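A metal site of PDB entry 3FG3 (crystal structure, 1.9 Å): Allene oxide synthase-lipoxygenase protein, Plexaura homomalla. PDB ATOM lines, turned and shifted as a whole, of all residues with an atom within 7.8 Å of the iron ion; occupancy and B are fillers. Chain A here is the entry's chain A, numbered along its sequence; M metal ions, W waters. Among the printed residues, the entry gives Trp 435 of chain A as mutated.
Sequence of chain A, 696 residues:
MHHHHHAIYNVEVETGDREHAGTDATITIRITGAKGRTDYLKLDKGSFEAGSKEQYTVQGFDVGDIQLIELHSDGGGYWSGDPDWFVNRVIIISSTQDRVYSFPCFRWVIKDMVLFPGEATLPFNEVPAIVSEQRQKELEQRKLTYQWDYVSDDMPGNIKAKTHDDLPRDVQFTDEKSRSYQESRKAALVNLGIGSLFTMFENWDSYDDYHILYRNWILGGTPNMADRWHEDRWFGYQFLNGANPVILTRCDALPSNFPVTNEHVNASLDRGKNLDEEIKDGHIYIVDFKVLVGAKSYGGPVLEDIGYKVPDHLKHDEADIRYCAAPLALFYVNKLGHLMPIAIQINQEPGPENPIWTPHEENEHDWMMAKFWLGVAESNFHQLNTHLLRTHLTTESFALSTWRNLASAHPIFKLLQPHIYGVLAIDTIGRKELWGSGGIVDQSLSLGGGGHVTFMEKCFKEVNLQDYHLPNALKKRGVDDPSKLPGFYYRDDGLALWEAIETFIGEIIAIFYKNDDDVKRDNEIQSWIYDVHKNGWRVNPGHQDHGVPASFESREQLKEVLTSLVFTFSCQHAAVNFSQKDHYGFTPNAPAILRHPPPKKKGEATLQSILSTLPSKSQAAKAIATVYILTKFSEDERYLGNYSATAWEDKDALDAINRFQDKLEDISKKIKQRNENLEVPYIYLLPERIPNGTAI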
ATOM      1  N   GLN A 383       0.929  -8.626  26.702  1.00  0.00           N
ATOM      2  CA  GLN A 383       0.518  -7.211  26.694  1.00  0.00           C
ATOM      3  C   GLN A 383       0.153  -6.736  28.090  1.00  0.00           C
ATOM      4  O   GLN A 383       0.549  -5.608  28.542  1.00  0.00           O
ATOM      5  CB  GLN A 383      -0.667  -7.007  25.738  1.00  0.00           C
ATOM      6  CG  GLN A 383      -0.815  -5.527  25.304  1.00  0.00           C
ATOM      7  CD  GLN A 383       0.394  -5.000  24.506  1.00  0.00           C
ATOM      8  OE1 GLN A 383       1.266  -4.325  25.036  1.00  0.00           O
ATOM      9  NE2 GLN A 383       0.421  -5.287  23.229  1.00  0.00           N
ATOM     10  N   HIS A 387       4.215  -6.663  29.827  1.00  0.00           N
ATOM     11  CA  HIS A 387       4.411  -5.254  29.467  1.00  0.00           C
ATOM     12  C   HIS A 387       3.643  -4.288  30.376  1.00  0.00           C
ATOM     13  O   HIS A 387       4.290  -3.581  31.142  1.00  0.00           O
ATOM     14  CB  HIS A 387       4.052  -5.014  27.988  1.00  0.00           C
ATOM     15  CG  HIS A 387       4.071  -3.582  27.578  1.00  0.00           C
ATOM     16  ND1 HIS A 387       3.077  -3.062  26.796  1.00  0.00           N
ATOM     17  CD2 HIS A 387       4.983  -2.596  27.764  1.00  0.00           C
ATOM     18  CE1 HIS A 387       3.364  -1.779  26.546  1.00  0.00           C
ATOM     19  NE2 HIS A 387       4.532  -1.490  27.096  1.00  0.00           N
ATOM     20  N   LEU A 388       2.293  -4.210  30.274  1.00  0.00           N
ATOM     21  CA  LEU A 388       1.555  -3.138  31.020  1.00  0.00           C
ATOM     22  C   LEU A 388       1.792  -3.196  32.521  1.00  0.00           C
ATOM     23  O   LEU A 388       2.202  -2.200  33.115  1.00  0.00           O
ATOM     24  CB  LEU A 388       0.049  -3.185  30.713  1.00  0.00           C
ATOM     25  CG  LEU A 388      -0.792  -2.057  31.299  1.00  0.00           C
ATOM     26  CD1 LEU A 388      -0.087  -0.685  31.083  1.00  0.00           C
ATOM     27  CD2 LEU A 388      -2.189  -2.063  30.659  1.00  0.00           C
ATOM     28  N   THR A 391       5.991  -3.485  33.706  1.00  0.00           N
ATOM     29  CA  THR A 391       6.886  -2.356  33.407  1.00  0.00           C
ATOM     30  C   THR A 391       6.103  -1.102  33.883  1.00  0.00           C
ATOM     31  O   THR A 391       6.150  -0.807  35.119  1.00  0.00           O
ATOM     32  CB  THR A 391       7.458  -2.309  31.947  1.00  0.00           C
ATOM     33  OG1 THR A 391       6.399  -2.181  30.976  1.00  0.00           O
ATOM     34  CG2 THR A 391       8.304  -3.619  31.642  1.00  0.00           C
ATOM     35  N   HIS A 392       5.306  -0.501  32.991  1.00  0.00           N
ATOM     36  CA  HIS A 392       4.487   0.671  33.335  1.00  0.00           C
ATOM     37  C   HIS A 392       3.911   0.723  34.760  1.00  0.00           C
ATOM     38  O   HIS A 392       4.306   1.561  35.519  1.00  0.00           O
ATOM     39  CB  HIS A 392       3.294   0.715  32.369  1.00  0.00           C
ATOM     40  CG  HIS A 392       3.680   1.086  30.979  1.00  0.00           C
ATOM     41  ND1 HIS A 392       3.565   2.371  30.534  1.00  0.00           N
ATOM     42  CD2 HIS A 392       4.141   0.348  29.934  1.00  0.00           C
ATOM     43  CE1 HIS A 392       3.956   2.442  29.263  1.00  0.00           C
ATOM     44  NE2 HIS A 392       4.302   1.217  28.869  1.00  0.00           N
ATOM     45  N   ILE A 426       2.593   8.797  30.521  1.00  0.00           N
ATOM     46  CA  ILE A 426       1.944   7.822  29.625  1.00  0.00           C
ATOM     47  C   ILE A 426       0.911   7.023  30.381  1.00  0.00           C
ATOM     48  O   ILE A 426      -0.160   6.627  29.794  1.00  0.00           O
ATOM     49  CB  ILE A 426       3.006   6.859  28.858  1.00  0.00           C
ATOM     50  CG1 ILE A 426       2.305   5.936  27.841  1.00  0.00           C
ATOM     51  CG2 ILE A 426       3.792   5.971  29.856  1.00  0.00           C
ATOM     52  CD1 ILE A 426       1.521   6.731  26.773  1.00  0.00           C
ATOM     53  N   ASP A 427       1.137   6.776  31.670  1.00  0.00           N
ATOM     54  CA  ASP A 427       0.131   5.950  32.367  1.00  0.00           C
ATOM     55  C   ASP A 427      -1.143   6.716  32.665  1.00  0.00           C
ATOM     56  O   ASP A 427      -2.265   6.124  32.675  1.00  0.00           O
ATOM     57  CB  ASP A 427       0.684   5.455  33.707  1.00  0.00           C
ATOM     58  CG  ASP A 427       1.632   4.245  33.519  1.00  0.00           C
ATOM     59  OD1 ASP A 427       1.971   3.905  32.341  1.00  0.00           O
ATOM     60  OD2 ASP A 427       2.096   3.685  34.553  1.00  0.00           O
ATOM     61  N   TRP A 435      -5.693   1.531  27.885  1.00  0.00           N
ATOM     62  CA  TRP A 435      -6.088   0.272  28.465  1.00  0.00           C
ATOM     63  C   TRP A 435      -7.215   0.503  29.432  1.00  0.00           C
ATOM     64  O   TRP A 435      -7.671  -0.402  30.108  1.00  0.00           O
ATOM     65  CB  TRP A 435      -4.867  -0.402  29.148  1.00  0.00           C
ATOM     66  CG  TRP A 435      -4.169   0.497  30.170  1.00  0.00           C
ATOM     67  CD1 TRP A 435      -4.528   0.695  31.465  1.00  0.00           C
ATOM     68  CD2 TRP A 435      -2.958   1.222  29.957  1.00  0.00           C
ATOM     69  NE1 TRP A 435      -3.603   1.512  32.084  1.00  0.00           N
ATOM     70  CE2 TRP A 435      -2.661   1.882  31.169  1.00  0.00           C
ATOM     71  CE3 TRP A 435      -2.106   1.401  28.851  1.00  0.00           C
ATOM     72  CZ2 TRP A 435      -1.522   2.681  31.321  1.00  0.00           C
ATOM     73  CZ3 TRP A 435      -0.981   2.209  29.000  1.00  0.00           C
ATOM     74  CH2 TRP A 435      -0.705   2.840  30.220  1.00  0.00           C
ATOM     75  N   HIS A 573      11.532  -2.682  29.646  1.00  0.00           N
ATOM     76  CA  HIS A 573      10.454  -2.121  28.879  1.00  0.00           C
ATOM     77  C   HIS A 573      10.793  -2.150  27.368  1.00  0.00           C
ATOM     78  O   HIS A 573       9.903  -2.482  26.520  1.00  0.00           O
ATOM     79  CB  HIS A 573      10.093  -0.670  29.362  1.00  0.00           C
ATOM     80  CG  HIS A 573       9.061  -0.025  28.476  1.00  0.00           C
ATOM     81  ND1 HIS A 573       9.362   0.977  27.549  1.00  0.00           N
ATOM     82  CD2 HIS A 573       7.727  -0.265  28.366  1.00  0.00           C
ATOM     83  CE1 HIS A 573       8.238   1.326  26.929  1.00  0.00           C
ATOM     84  NE2 HIS A 573       7.247   0.566  27.381  1.00  0.00           N
ATOM     85  N   ALA A 574      12.022  -1.721  26.990  1.00  0.00           N
ATOM     86  CA  ALA A 574      12.397  -1.725  25.583  1.00  0.00           C
ATOM     87  C   ALA A 574      12.241  -3.161  24.985  1.00  0.00           C
ATOM     88  O   ALA A 574      11.669  -3.312  23.879  1.00  0.00           O
ATOM     89  CB  ALA A 574      13.835  -1.218  25.393  1.00  0.00           C
ATOM     90  N   VAL A 576      10.411  -5.730  25.829  1.00  0.00           N
ATOM     91  CA  VAL A 576       9.056  -6.292  25.732  1.00  0.00           C
ATOM     92  C   VAL A 576       8.105  -5.352  24.980  1.00  0.00           C
ATOM     93  O   VAL A 576       6.975  -5.755  24.657  1.00  0.00           O
ATOM     94  CB  VAL A 576       8.516  -6.706  27.090  1.00  0.00           C
ATOM     95  CG1 VAL A 576       9.582  -7.676  27.842  1.00  0.00           C
ATOM     96  CG2 VAL A 576       8.128  -5.383  27.923  1.00  0.00           C
ATOM     97  N   ASN A 577       8.580  -4.132  24.625  1.00  0.00           N
ATOM     98  CA  ASN A 577       7.705  -3.138  23.953  1.00  0.00           C
ATOM     99  C   ASN A 577       8.124  -2.883  22.511  1.00  0.00           C
ATOM    100  O   ASN A 577       7.310  -3.020  21.587  1.00  0.00           O
ATOM    101  CB  ASN A 577       7.605  -1.788  24.732  1.00  0.00           C
ATOM    102  CG  ASN A 577       6.701  -0.805  24.011  1.00  0.00           C
ATOM    103  OD1 ASN A 577       7.158   0.244  23.484  1.00  0.00           O
ATOM    104  ND2 ASN A 577       5.442  -1.136  23.929  1.00  0.00           N
ATOM    105  N   PHE A 578       9.385  -2.515  22.300  1.00  0.00           N
ATOM    106  CA  PHE A 578       9.780  -2.172  20.964  1.00  0.00           C
ATOM    107  C   PHE A 578       9.949  -3.399  20.028  1.00  0.00           C
ATOM    108  O   PHE A 578      10.114  -3.209  18.802  1.00  0.00           O
ATOM    109  CB  PHE A 578      10.984  -1.204  20.951  1.00  0.00           C
ATOM    110  CG  PHE A 578      10.672   0.063  21.714  1.00  0.00           C
ATOM    111  CD1 PHE A 578      11.254   0.284  22.967  1.00  0.00           C
ATOM    112  CD2 PHE A 578       9.742   0.977  21.176  1.00  0.00           C
ATOM    113  CE1 PHE A 578      10.937   1.428  23.739  1.00  0.00           C
ATOM    114  CE2 PHE A 578       9.411   2.133  21.902  1.00  0.00           C
ATOM    115  CZ  PHE A 578       9.963   2.358  23.219  1.00  0.00           C
ATOM    116  N   GLN A 580       7.540  -5.230  19.534  1.00  0.00           N
ATOM    117  CA  GLN A 580       6.177  -5.596  19.116  1.00  0.00           C
ATOM    118  C   GLN A 580       5.875  -5.517  17.639  1.00  0.00           C
ATOM    119  O   GLN A 580       4.969  -6.226  17.153  1.00  0.00           O
ATOM    120  CB  GLN A 580       5.138  -4.745  19.844  1.00  0.00           C
ATOM    121  CG  GLN A 580       5.025  -5.219  21.330  1.00  0.00           C
ATOM    122  CD  GLN A 580       4.007  -4.351  22.024  1.00  0.00           C
ATOM    123  OE1 GLN A 580       4.288  -3.193  22.378  1.00  0.00           O
ATOM    124  NE2 GLN A 580       2.817  -4.842  22.104  1.00  0.00           N
ATOM    125  N   LEU A 630       2.085   2.285  20.405  1.00  0.00           N
ATOM    126  CA  LEU A 630       2.894   1.911  21.618  1.00  0.00           C
ATOM    127  C   LEU A 630       4.331   1.810  21.342  1.00  0.00           C
ATOM    128  O   LEU A 630       5.133   1.683  22.302  1.00  0.00           O
ATOM    129  CB  LEU A 630       2.416   0.563  22.185  1.00  0.00           C
ATOM    130  CG  LEU A 630       0.921   0.530  22.656  1.00  0.00           C
ATOM    131  CD1 LEU A 630       0.633  -0.883  23.280  1.00  0.00           C
ATOM    132  CD2 LEU A 630       0.522   1.630  23.689  1.00  0.00           C
ATOM    133  N   THR A 631       4.733   1.815  20.081  1.00  0.00           N
ATOM    134  CA  THR A 631       6.141   1.644  19.772  1.00  0.00           C
ATOM    135  C   THR A 631       6.823   2.799  19.047  1.00  0.00           C
ATOM    136  O   THR A 631       8.008   2.671  18.599  1.00  0.00           O
ATOM    137  CB  THR A 631       6.424   0.380  18.921  1.00  0.00           C
ATOM    138  OG1 THR A 631       5.800   0.489  17.623  1.00  0.00           O
ATOM    139  CG2 THR A 631       5.894  -0.834  19.629  1.00  0.00           C
ATOM    140  N   GLY A 693      13.768   5.668  29.704  1.00  0.00           N
ATOM    141  CA  GLY A 693      12.599   5.497  30.526  1.00  0.00           C
ATOM    142  C   GLY A 693      11.461   4.771  29.822  1.00  0.00           C
ATOM    143  O   GLY A 693      11.600   4.268  28.679  1.00  0.00           O
ATOM    144  N   THR A 694      10.379   4.639  30.555  1.00  0.00           N
ATOM    145  CA  THR A 694       9.161   3.966  30.051  1.00  0.00           C
ATOM    146  C   THR A 694       8.176   5.076  29.725  1.00  0.00           C
ATOM    147  O   THR A 694       7.526   5.602  30.636  1.00  0.00           O
ATOM    148  CB  THR A 694       8.603   3.023  31.146  1.00  0.00           C
ATOM    149  OG1 THR A 694       9.542   1.991  31.313  1.00  0.00           O
ATOM    150  CG2 THR A 694       7.210   2.358  30.728  1.00  0.00           C
ATOM    151  N   ALA A 695       8.120   5.483  28.453  1.00  0.00           N
ATOM    152  CA  ALA A 695       7.417   6.752  28.121  1.00  0.00           C
ATOM    153  C   ALA A 695       6.323   6.543  27.076  1.00  0.00           C
ATOM    154  O   ALA A 695       5.677   7.504  26.640  1.00  0.00           O
ATOM    155  CB  ALA A 695       8.440   7.788  27.641  1.00  0.00           C
ATOM    156  N   ILE A 696       6.184   5.291  26.611  1.00  0.00           N
ATOM    157  CA  ILE A 696       5.198   5.013  25.579  1.00  0.00           C
ATOM    158  C   ILE A 696       4.786   3.534  25.724  1.00  0.00           C
ATOM    159  O   ILE A 696       3.770   3.039  25.114  1.00  0.00           O
ATOM    160  CB  ILE A 696       5.783   5.317  24.133  1.00  0.00           C
ATOM    161  CG1 ILE A 696       4.666   5.384  23.054  1.00  0.00           C
ATOM    162  CG2 ILE A 696       6.922   4.233  23.764  1.00  0.00           C
ATOM    163  CD1 ILE A 696       3.577   6.424  23.300  1.00  0.00           C
ATOM    164  OXT ILE A 696       5.492   2.791  26.440  1.00  0.00           O
HETATM  165 FE    FE M   1       5.181   0.665  26.988  1.00  0.00          FE
HETATM  166  O   HOH W   1       3.940   0.691  25.263  1.00  0.00           O
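The iron ion is bound by NE2 of His 573, water W1, NE2 of His 392, OXT of Ile 696 and NE2 of His 387.
The iron ion has five donor atoms within binding distance.
Water W1 bridges the side-chain amide nitrogen (ND2) of Asn 577 (2.7 Å) and the backbone carbonyl oxygen (O) of Leu 630 (3.3 Å).
A ring nitrogen (ND1) of His 387 is in hydrogen-bond range of the side-chain amide oxygen (OE1) of Gln 383 (2.8 Å).
OD1 of Asp 427 is in hydrogen-bond range of ND1 of His 392, at 2.9 Å.
The side-chain hydroxyl (OG1) of Thr 391 sits at hydrogen-bond distance from the backbone carbonyl oxygen (O) of His 387, 2.5 Å away.
O of Leu 630 sits close to OD1 of Asn 577 (2.8 Å).
ND2 of Asn 577 sits close to NE2 of His 387 (3.3 Å).
The side-chain amide nitrogen (ND2) of Asn 577 lies within hydrogen-bond range of the side-chain amide oxygen (OE1) of Gln 580, at 2.8 Å.
Merely in contact with the iron ion: Asn 577 (3.6 Å).
Within 4 Å of the iron ion: His 387, His 392, His 573, Asn 577 and Ile 696.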
